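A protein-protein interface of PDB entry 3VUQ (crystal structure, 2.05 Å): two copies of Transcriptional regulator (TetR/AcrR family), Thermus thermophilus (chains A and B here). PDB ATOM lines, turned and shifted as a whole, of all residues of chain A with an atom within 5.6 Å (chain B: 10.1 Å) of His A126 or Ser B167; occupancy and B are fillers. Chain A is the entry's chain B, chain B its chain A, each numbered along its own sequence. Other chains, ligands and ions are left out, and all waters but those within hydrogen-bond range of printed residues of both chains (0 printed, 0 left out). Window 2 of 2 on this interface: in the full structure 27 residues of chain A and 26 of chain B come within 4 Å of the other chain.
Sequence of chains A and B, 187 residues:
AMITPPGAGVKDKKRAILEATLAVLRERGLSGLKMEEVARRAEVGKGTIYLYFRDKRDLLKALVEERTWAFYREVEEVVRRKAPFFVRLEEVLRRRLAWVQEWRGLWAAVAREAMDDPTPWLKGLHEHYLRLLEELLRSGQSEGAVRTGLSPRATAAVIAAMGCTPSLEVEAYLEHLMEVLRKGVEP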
ATOM      1  N   TYR A  72     -25.080  11.515 -12.186  1.00  0.00           N
ATOM      2  CA  TYR A  72     -26.178  12.183 -12.873  1.00  0.00           C
ATOM      3  C   TYR A  72     -27.532  11.950 -12.230  1.00  0.00           C
ATOM      4  O   TYR A  72     -28.377  12.842 -12.213  1.00  0.00           O
ATOM      5  CB  TYR A  72     -26.215  11.748 -14.331  1.00  0.00           C
ATOM      6  CG  TYR A  72     -25.084  12.331 -15.128  1.00  0.00           C
ATOM      7  CD1 TYR A  72     -24.706  13.665 -14.956  1.00  0.00           C
ATOM      8  CD2 TYR A  72     -24.412  11.575 -16.079  1.00  0.00           C
ATOM      9  CE1 TYR A  72     -23.687  14.228 -15.716  1.00  0.00           C
ATOM     10  CE2 TYR A  72     -23.392  12.127 -16.843  1.00  0.00           C
ATOM     11  CZ  TYR A  72     -23.035  13.452 -16.658  1.00  0.00           C
ATOM     12  OH  TYR A  72     -22.031  14.001 -17.419  1.00  0.00           O
ATOM     13  N   ARG A  96     -21.193  18.606  -7.415  1.00  0.00           N
ATOM     14  CA  ARG A  96     -20.300  18.654  -8.552  1.00  0.00           C
ATOM     15  C   ARG A  96     -18.838  18.745  -8.083  1.00  0.00           C
ATOM     16  O   ARG A  96     -17.947  18.109  -8.648  1.00  0.00           O
ATOM     17  CB  ARG A  96     -20.622  19.884  -9.408  1.00  0.00           C
ATOM     18  CG  ARG A  96     -19.672  20.087 -10.550  1.00  0.00           C
ATOM     19  CD  ARG A  96     -19.853  19.029 -11.593  1.00  0.00           C
ATOM     20  NE  ARG A  96     -18.896  19.198 -12.677  1.00  0.00           N
ATOM     21  CZ  ARG A  96     -18.803  18.381 -13.721  1.00  0.00           C
ATOM     22  NH1 ARG A  96     -19.615  17.334 -13.827  1.00  0.00           N
ATOM     23  NH2 ARG A  96     -17.885  18.599 -14.651  1.00  0.00           N
ATOM     24  N   LEU A 122     -16.040  11.688 -23.163  1.00  0.00           N
ATOM     25  CA  LEU A 122     -16.129  12.595 -22.034  1.00  0.00           C
ATOM     26  C   LEU A 122     -16.940  13.828 -22.408  1.00  0.00           C
ATOM     27  O   LEU A 122     -17.662  14.372 -21.579  1.00  0.00           O
ATOM     28  CB  LEU A 122     -14.728  12.988 -21.545  1.00  0.00           C
ATOM     29  CG  LEU A 122     -13.847  11.807 -21.106  1.00  0.00           C
ATOM     30  CD1 LEU A 122     -12.656  12.314 -20.319  1.00  0.00           C
ATOM     31  CD2 LEU A 122     -14.655  10.846 -20.244  1.00  0.00           C
ATOM     32  N   LYS A 123     -16.824  14.267 -23.656  1.00  0.00           N
ATOM     33  CA  LYS A 123     -17.584  15.419 -24.105  1.00  0.00           C
ATOM     34  C   LYS A 123     -19.059  15.046 -23.961  1.00  0.00           C
ATOM     35  O   LYS A 123     -19.881  15.856 -23.520  1.00  0.00           O
ATOM     36  CB  LYS A 123     -17.254  15.747 -25.563  1.00  0.00           C
ATOM     37  CG  LYS A 123     -17.828  17.071 -26.034  1.00  0.00           C
ATOM     38  CD  LYS A 123     -17.478  17.351 -27.486  1.00  0.00           C
ATOM     39  CE  LYS A 123     -18.027  18.697 -27.929  1.00  0.00           C
ATOM     40  NZ  LYS A 123     -17.750  18.971 -29.365  1.00  0.00           N
ATOM     41  N   GLY A 124     -19.381  13.806 -24.317  1.00  0.00           N
ATOM     42  CA  GLY A 124     -20.746  13.331 -24.207  1.00  0.00           C
ATOM     43  C   GLY A 124     -21.263  13.423 -22.781  1.00  0.00           C
ATOM     44  O   GLY A 124     -22.464  13.516 -22.556  1.00  0.00           O
ATOM     45  N   LEU A 125     -20.360  13.379 -21.807  1.00  0.00           N
ATOM     46  CA  LEU A 125     -20.764  13.479 -20.409  1.00  0.00           C
ATOM     47  C   LEU A 125     -21.006  14.947 -20.081  1.00  0.00           C
ATOM     48  O   LEU A 125     -22.042  15.298 -19.518  1.00  0.00           O
ATOM     49  CB  LEU A 125     -19.688  12.889 -19.495  1.00  0.00           C
ATOM     50  CG  LEU A 125     -19.367  11.408 -19.759  1.00  0.00           C
ATOM     51  CD1 LEU A 125     -18.351  10.901 -18.738  1.00  0.00           C
ATOM     52  CD2 LEU A 125     -20.640  10.583 -19.693  1.00  0.00           C
ATOM     53  N   HIS A 126     -20.059  15.805 -20.448  1.00  0.00           N
ATOM     54  CA  HIS A 126     -20.201  17.237 -20.209  1.00  0.00           C
ATOM     55  C   HIS A 126     -21.616  17.642 -20.647  1.00  0.00           C
ATOM     56  O   HIS A 126     -22.255  18.497 -20.031  1.00  0.00           O
ATOM     57  CB  HIS A 126     -19.155  18.012 -21.023  1.00  0.00           C
ATOM     58  CG  HIS A 126     -19.124  19.485 -20.739  1.00  0.00           C
ATOM     59  ND1 HIS A 126     -19.061  19.996 -19.460  1.00  0.00           N
ATOM     60  CD2 HIS A 126     -19.126  20.555 -21.572  1.00  0.00           C
ATOM     61  CE1 HIS A 126     -19.029  21.317 -19.517  1.00  0.00           C
ATOM     62  NE2 HIS A 126     -19.067  21.681 -20.787  1.00  0.00           N
ATOM     63  N   GLU A 127     -22.098  16.998 -21.708  1.00  0.00           N
ATOM     64  CA  GLU A 127     -23.429  17.260 -22.251  1.00  0.00           C
ATOM     65  C   GLU A 127     -24.568  16.965 -21.281  1.00  0.00           C
ATOM     66  O   GLU A 127     -25.396  17.835 -21.007  1.00  0.00           O
ATOM     67  CB  GLU A 127     -23.650  16.445 -23.527  1.00  0.00           C
ATOM     68  CG  GLU A 127     -22.848  16.925 -24.713  1.00  0.00           C
ATOM     69  CD  GLU A 127     -23.066  18.397 -24.993  1.00  0.00           C
ATOM     70  OE1 GLU A 127     -24.237  18.826 -25.054  1.00  0.00           O
ATOM     71  OE2 GLU A 127     -22.064  19.125 -25.160  1.00  0.00           O
ATOM     72  N   HIS A 128     -24.622  15.742 -20.767  1.00  0.00           N
ATOM     73  CA  HIS A 128     -25.686  15.383 -19.846  1.00  0.00           C
ATOM     74  C   HIS A 128     -25.755  16.367 -18.661  1.00  0.00           C
ATOM     75  O   HIS A 128     -26.844  16.769 -18.246  1.00  0.00           O
ATOM     76  CB  HIS A 128     -25.497  13.943 -19.360  1.00  0.00           C
ATOM     77  CG  HIS A 128     -26.723  13.348 -18.738  1.00  0.00           C
ATOM     78  ND1 HIS A 128     -26.800  12.023 -18.366  1.00  0.00           N
ATOM     79  CD2 HIS A 128     -27.913  13.902 -18.401  1.00  0.00           C
ATOM     80  CE1 HIS A 128     -27.983  11.787 -17.824  1.00  0.00           C
ATOM     81  NE2 HIS A 128     -28.676  12.912 -17.833  1.00  0.00           N
ATOM     82  N   TYR A 129     -24.602  16.773 -18.133  1.00  0.00           N
ATOM     83  CA  TYR A 129     -24.580  17.718 -17.017  1.00  0.00           C
ATOM     84  C   TYR A 129     -25.168  19.067 -17.467  1.00  0.00           C
ATOM     85  O   TYR A 129     -25.951  19.669 -16.747  1.00  0.00           O
ATOM     86  CB  TYR A 129     -23.140  17.909 -16.506  1.00  0.00           C
ATOM     87  CG  TYR A 129     -22.990  18.849 -15.318  1.00  0.00           C
ATOM     88  CD1 TYR A 129     -23.729  18.662 -14.155  1.00  0.00           C
ATOM     89  CD2 TYR A 129     -22.074  19.901 -15.349  1.00  0.00           C
ATOM     90  CE1 TYR A 129     -23.565  19.487 -13.064  1.00  0.00           C
ATOM     91  CE2 TYR A 129     -21.899  20.732 -14.255  1.00  0.00           C
ATOM     92  CZ  TYR A 129     -22.644  20.526 -13.120  1.00  0.00           C
ATOM     93  OH  TYR A 129     -22.499  21.370 -12.037  1.00  0.00           O
ATOM     94  N   LEU A 130     -24.793  19.513 -18.661  1.00  0.00           N
ATOM     95  CA  LEU A 130     -25.261  20.781 -19.219  1.00  0.00           C
ATOM     96  C   LEU A 130     -26.770  20.827 -19.402  1.00  0.00           C
ATOM     97  O   LEU A 130     -27.394  21.866 -19.186  1.00  0.00           O
ATOM     98  CB  LEU A 130     -24.595  21.053 -20.573  1.00  0.00           C
ATOM     99  CG  LEU A 130     -23.228  21.739 -20.588  1.00  0.00           C
ATOM    100  CD1 LEU A 130     -22.742  21.841 -22.017  1.00  0.00           C
ATOM    101  CD2 LEU A 130     -23.325  23.120 -19.964  1.00  0.00           C
ATOM    102  N   ARG A 131     -27.342  19.701 -19.813  1.00  0.00           N
ATOM    103  CA  ARG A 131     -28.772  19.583 -20.039  1.00  0.00           C
ATOM    104  C   ARG A 131     -29.470  19.681 -18.690  1.00  0.00           C
ATOM    105  O   ARG A 131     -30.536  20.279 -18.580  1.00  0.00           O
ATOM    106  CB  ARG A 131     -29.088  18.243 -20.717  1.00  0.00           C
ATOM    107  CG  ARG A 131     -30.502  18.111 -21.266  1.00  0.00           C
ATOM    108  CD  ARG A 131     -30.735  16.723 -21.870  1.00  0.00           C
ATOM    109  NE  ARG A 131     -32.023  16.612 -22.554  1.00  0.00           N
ATOM    110  CZ  ARG A 131     -33.207  16.764 -21.964  1.00  0.00           C
ATOM    111  NH1 ARG A 131     -33.281  17.037 -20.667  1.00  0.00           N
ATOM    112  NH2 ARG A 131     -34.319  16.645 -22.675  1.00  0.00           N
ATOM    113  N   ALA A 157     -23.763  26.739 -19.648  1.00  0.00           N
ATOM    114  CA  ALA A 157     -22.351  26.614 -20.010  1.00  0.00           C
ATOM    115  C   ALA A 157     -21.494  27.420 -19.034  1.00  0.00           C
ATOM    116  O   ALA A 157     -20.446  26.954 -18.584  1.00  0.00           O
ATOM    117  CB  ALA A 157     -22.115  27.109 -21.439  1.00  0.00           C
ATOM    118  N   ALA A 160     -21.406  25.628 -15.708  1.00  0.00           N
ATOM    119  CA  ALA A 160     -20.547  24.451 -15.830  1.00  0.00           C
ATOM    120  C   ALA A 160     -19.078  24.881 -15.646  1.00  0.00           C
ATOM    121  O   ALA A 160     -18.315  24.227 -14.937  1.00  0.00           O
ATOM    122  CB  ALA A 160     -20.744  23.793 -17.197  1.00  0.00           C
ATOM    123  N   ALA A 161     -18.687  25.985 -16.279  1.00  0.00           N
ATOM    124  CA  ALA A 161     -17.318  26.495 -16.160  1.00  0.00           C
ATOM    125  C   ALA A 161     -17.054  27.039 -14.753  1.00  0.00           C
ATOM    126  O   ALA A 161     -16.302  26.442 -13.982  1.00  0.00           O
ATOM    127  CB  ALA A 161     -17.063  27.599 -17.200  1.00  0.00           C
ATOM    128  N   LEU B  97      -8.469  32.418 -21.198  1.00  0.00           N
ATOM    129  CA  LEU B  97      -9.061  31.321 -21.959  1.00  0.00           C
ATOM    130  C   LEU B  97      -8.072  30.850 -23.036  1.00  0.00           C
ATOM    131  O   LEU B  97      -7.869  29.651 -23.215  1.00  0.00           O
ATOM    132  CB  LEU B  97     -10.379  31.781 -22.612  1.00  0.00           C
ATOM    133  CG  LEU B  97     -11.540  32.006 -21.632  1.00  0.00           C
ATOM    134  CD1 LEU B  97     -12.728  32.616 -22.351  1.00  0.00           C
ATOM    135  CD2 LEU B  97     -11.925  30.680 -20.987  1.00  0.00           C
ATOM    136  N   GLN B 101      -5.950  27.006 -23.055  1.00  0.00           N
ATOM    137  CA  GLN B 101      -5.922  26.163 -24.242  1.00  0.00           C
ATOM    138  C   GLN B 101      -4.499  25.879 -24.706  1.00  0.00           C
ATOM    139  O   GLN B 101      -4.188  24.797 -25.195  1.00  0.00           O
ATOM    140  CB  GLN B 101      -6.692  26.841 -25.374  1.00  0.00           C
ATOM    141  CG  GLN B 101      -6.736  26.033 -26.649  1.00  0.00           C
ATOM    142  CD  GLN B 101      -7.816  26.506 -27.589  1.00  0.00           C
ATOM    143  OE1 GLN B 101      -7.828  27.664 -28.007  1.00  0.00           O
ATOM    144  NE2 GLN B 101      -8.737  25.613 -27.927  1.00  0.00           N
ATOM    145  N   MET B 162     -12.578  29.732 -14.083  1.00  0.00           N
ATOM    146  CA  MET B 162     -12.777  29.396 -15.495  1.00  0.00           C
ATOM    147  C   MET B 162     -11.612  28.543 -16.009  1.00  0.00           C
ATOM    148  O   MET B 162     -10.486  28.679 -15.530  1.00  0.00           O
ATOM    149  CB  MET B 162     -12.873  30.672 -16.341  1.00  0.00           C
ATOM    150  CG  MET B 162     -13.740  31.766 -15.738  1.00  0.00           C
ATOM    151  SD  MET B 162     -15.360  31.212 -15.171  1.00  0.00           S
ATOM    152  CE  MET B 162     -15.084  31.126 -13.372  1.00  0.00           C
ATOM    153  N   GLY B 163     -11.874  27.659 -16.968  1.00  0.00           N
ATOM    154  CA  GLY B 163     -10.786  26.860 -17.510  1.00  0.00           C
ATOM    155  C   GLY B 163     -10.912  25.348 -17.637  1.00  0.00           C
ATOM    156  O   GLY B 163     -10.049  24.722 -18.258  1.00  0.00           O
ATOM    157  N   CYS B 164     -11.958  24.750 -17.073  1.00  0.00           N
ATOM    158  CA  CYS B 164     -12.117  23.297 -17.157  1.00  0.00           C
ATOM    159  C   CYS B 164     -13.294  22.859 -18.025  1.00  0.00           C
ATOM    160  O   CYS B 164     -13.625  21.673 -18.073  1.00  0.00           O
ATOM    161  CB  CYS B 164     -12.287  22.699 -15.759  1.00  0.00           C
ATOM    162  SG  CYS B 164     -13.992  22.726 -15.105  1.00  0.00           S
ATOM    163  N   THR B 165     -13.924  23.808 -18.708  1.00  0.00           N
ATOM    164  CA  THR B 165     -15.065  23.490 -19.557  1.00  0.00           C
ATOM    165  C   THR B 165     -14.911  24.046 -20.970  1.00  0.00           C
ATOM    166  O   THR B 165     -14.681  25.243 -21.157  1.00  0.00           O
ATOM    167  CB  THR B 165     -16.378  24.039 -18.959  1.00  0.00           C
ATOM    168  OG1 THR B 165     -16.304  25.468 -18.876  1.00  0.00           O
ATOM    169  CG2 THR B 165     -16.616  23.463 -17.570  1.00  0.00           C
ATOM    170  N   PRO B 166     -15.035  23.175 -21.985  1.00  0.00           N
ATOM    171  CA  PRO B 166     -14.915  23.571 -23.391  1.00  0.00           C
ATOM    172  C   PRO B 166     -16.162  24.309 -23.874  1.00  0.00           C
ATOM    173  O   PRO B 166     -16.269  24.664 -25.048  1.00  0.00           O
ATOM    174  CB  PRO B 166     -14.722  22.237 -24.100  1.00  0.00           C
ATOM    175  CG  PRO B 166     -15.577  21.321 -23.286  1.00  0.00           C
ATOM    176  CD  PRO B 166     -15.216  21.716 -21.870  1.00  0.00           C
ATOM    177  N   SER B 167     -17.102  24.529 -22.958  1.00  0.00           N
ATOM    178  CA  SER B 167     -18.349  25.222 -23.274  1.00  0.00           C
ATOM    179  C   SER B 167     -19.082  24.546 -24.429  1.00  0.00           C
ATOM    180  O   SER B 167     -19.519  23.399 -24.314  1.00  0.00           O
ATOM    181  CB  SER B 167     -18.062  26.686 -23.626  1.00  0.00           C
ATOM    182  OG  SER B 167     -17.436  27.357 -22.544  1.00  0.00           O
ATOM    183  N   VAL B 170     -15.557  31.432 -26.374  1.00  0.00           N
ATOM    184  CA  VAL B 170     -15.841  32.063 -27.659  1.00  0.00           C
ATOM    185  C   VAL B 170     -16.501  33.413 -27.419  1.00  0.00           C
ATOM    186  O   VAL B 170     -16.848  33.733 -26.292  1.00  0.00           O
ATOM    187  CB  VAL B 170     -16.798  31.202 -28.513  1.00  0.00           C
ATOM    188  CG1 VAL B 170     -16.196  29.821 -28.735  1.00  0.00           C
ATOM    189  CG2 VAL B 170     -18.160  31.107 -27.836  1.00  0.00           C
ATOM    190  N   GLU B 171     -16.679  34.192 -28.484  1.00  0.00           N
ATOM    191  CA  GLU B 171     -17.301  35.515 -28.386  1.00  0.00           C
ATOM    192  C   GLU B 171     -18.659  35.461 -27.684  1.00  0.00           C
ATOM    193  O   GLU B 171     -18.846  36.079 -26.635  1.00  0.00           O
ATOM    194  CB  GLU B 171     -17.468  36.129 -29.781  1.00  0.00           C
ATOM    195  CG  GLU B 171     -16.174  36.199 -30.580  1.00  0.00           C
ATOM    196  CD  GLU B 171     -15.147  37.126 -29.958  1.00  0.00           C
ATOM    197  OE1 GLU B 171     -14.960  37.065 -28.726  1.00  0.00           O
ATOM    198  OE2 GLU B 171     -14.517  37.908 -30.702  1.00  0.00           O
ATOM    199  N   ALA B 172     -19.604  34.726 -28.268  1.00  0.00           N
ATOM    200  CA  ALA B 172     -20.935  34.600 -27.682  1.00  0.00           C
ATOM    201  C   ALA B 172     -20.784  34.189 -26.233  1.00  0.00           C
ATOM    202  O   ALA B 172     -21.261  34.865 -25.330  1.00  0.00           O
ATOM    203  CB  ALA B 172     -21.751  33.550 -28.428  1.00  0.00           C
ATOM    204  N   TYR B 173     -20.103  33.071 -26.024  1.00  0.00           N
ATOM    205  CA  TYR B 173     -19.897  32.567 -24.686  1.00  0.00           C
ATOM    206  C   TYR B 173     -19.433  33.632 -23.693  1.00  0.00           C
ATOM    207  O   TYR B 173     -19.986  33.786 -22.614  1.00  0.00           O
ATOM    208  CB  TYR B 173     -18.859  31.456 -24.687  1.00  0.00           C
ATOM    209  CG  TYR B 173     -18.574  30.991 -23.283  1.00  0.00           C
ATOM    210  CD1 TYR B 173     -19.580  30.383 -22.525  1.00  0.00           C
ATOM    211  CD2 TYR B 173     -17.352  31.238 -22.676  1.00  0.00           C
ATOM    212  CE1 TYR B 173     -19.376  30.038 -21.193  1.00  0.00           C
ATOM    213  CE2 TYR B 173     -17.133  30.898 -21.329  1.00  0.00           C
ATOM    214  CZ  TYR B 173     -18.160  30.300 -20.597  1.00  0.00           C
ATOM    215  OH  TYR B 173     -17.995  29.985 -19.269  1.00  0.00           O
ATOM    216  N   LEU B 174     -18.391  34.351 -24.065  1.00  0.00           N
ATOM    217  CA  LEU B 174     -17.822  35.364 -23.196  1.00  0.00           C
ATOM    218  C   LEU B 174     -18.819  36.463 -22.806  1.00  0.00           C
ATOM    219  O   LEU B 174     -18.797  36.959 -21.675  1.00  0.00           O
ATOM    220  CB  LEU B 174     -16.604  35.965 -23.890  1.00  0.00           C
ATOM    221  CG  LEU B 174     -15.564  36.701 -23.053  1.00  0.00           C
ATOM    222  CD1 LEU B 174     -15.180  35.875 -21.826  1.00  0.00           C
ATOM    223  CD2 LEU B 174     -14.344  36.957 -23.935  1.00  0.00           C
ATOM    224  N   GLU B 175     -19.689  36.841 -23.737  1.00  0.00           N
ATOM    225  CA  GLU B 175     -20.670  37.892 -23.463  1.00  0.00           C
ATOM    226  C   GLU B 175     -21.640  37.453 -22.361  1.00  0.00           C
ATOM    227  O   GLU B 175     -22.043  38.255 -21.519  1.00  0.00           O
ATOM    228  CB  GLU B 175     -21.437  38.245 -24.748  1.00  0.00           C
ATOM    229  CG  GLU B 175     -20.570  38.726 -25.897  1.00  0.00           C
ATOM    230  CD  GLU B 175     -21.313  38.648 -27.235  1.00  0.00           C
ATOM    231  OE1 GLU B 175     -21.898  37.573 -27.521  1.00  0.00           O
ATOM    232  OE2 GLU B 175     -21.310  39.649 -27.994  1.00  0.00           O
ATOM    233  N   HIS B 176     -22.038  36.184 -22.393  1.00  0.00           N
ATOM    234  CA  HIS B 176     -22.927  35.641 -21.381  1.00  0.00           C
ATOM    235  C   HIS B 176     -22.206  35.547 -20.026  1.00  0.00           C
ATOM    236  O   HIS B 176     -22.790  35.826 -18.973  1.00  0.00           O
ATOM    237  CB  HIS B 176     -23.424  34.262 -21.822  1.00  0.00           C
ATOM    238  CG  HIS B 176     -24.338  34.308 -23.012  1.00  0.00           C
ATOM    239  ND1 HIS B 176     -25.674  34.629 -22.907  1.00  0.00           N
ATOM    240  CD2 HIS B 176     -24.112  34.053 -24.326  1.00  0.00           C
ATOM    241  CE1 HIS B 176     -26.236  34.566 -24.104  1.00  0.00           C
ATOM    242  NE2 HIS B 176     -25.310  34.218 -24.983  1.00  0.00           N
ATOM    243  N   LEU B 177     -20.942  35.144 -20.046  1.00  0.00           N
ATOM    244  CA  LEU B 177     -20.175  35.062 -18.796  1.00  0.00           C
ATOM    245  C   LEU B 177     -20.073  36.472 -18.180  1.00  0.00           C
ATOM    246  O   LEU B 177     -20.244  36.645 -16.972  1.00  0.00           O
ATOM    247  CB  LEU B 177     -18.766  34.531 -19.060  1.00  0.00           C
ATOM    248  CG  LEU B 177     -17.747  34.595 -17.895  1.00  0.00           C
ATOM    249  CD1 LEU B 177     -18.207  33.697 -16.706  1.00  0.00           C
ATOM    250  CD2 LEU B 177     -16.381  34.110 -18.396  1.00  0.00           C
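Among the printed residues, merely in contact across the chains: Ala A161 with Thr B165, Ala A160 with Thr B165, Ala A161 with Tyr B173, His A126 with Thr B165, His A126 with Ser B167 and Ala A157 with Tyr B173.
Gly A124 touches none of the printed residues of chain B. Of the printed residues of chain B, His A126 touches Thr B165 and Ser B167. Of the printed residues of chain B, Ala A157 touches Tyr B173 (3.96 Å). Of the printed residues of chain B, Ala A160 touches Thr B165. Of the printed residues of chain A, Thr B165 touches His A126, Ala A160 and Ala A161. Ser B167 touches one residue of chain A. Of the printed residues of chain A, Tyr B173 touches Ala A157 (3.96 Å) and Ala A161 (3.3 Å).
Of the 16 printed residues of chain B, 3 touch a printed residue of chain A. Hydrophobic or aromatic side chains of chain B within 4 Å of the printed part of chain A: Tyr B173. Of the 15 printed residues of chain A, 4 touch a printed residue of chain B. Hydrophobic or aromatic side chains of chain A within 4 Å of the printed part of chain B: His A126 and Ala A161. Along chain A the printed residues that touch a printed residue of chain B span positions 126 to 161. Among the printed residues, 6 pairs touch across the chains.
No position is printed for both chains. Of the 6 pairs that touch across the chains among the printed residues, none has its exchanged pair printed and touching as well.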
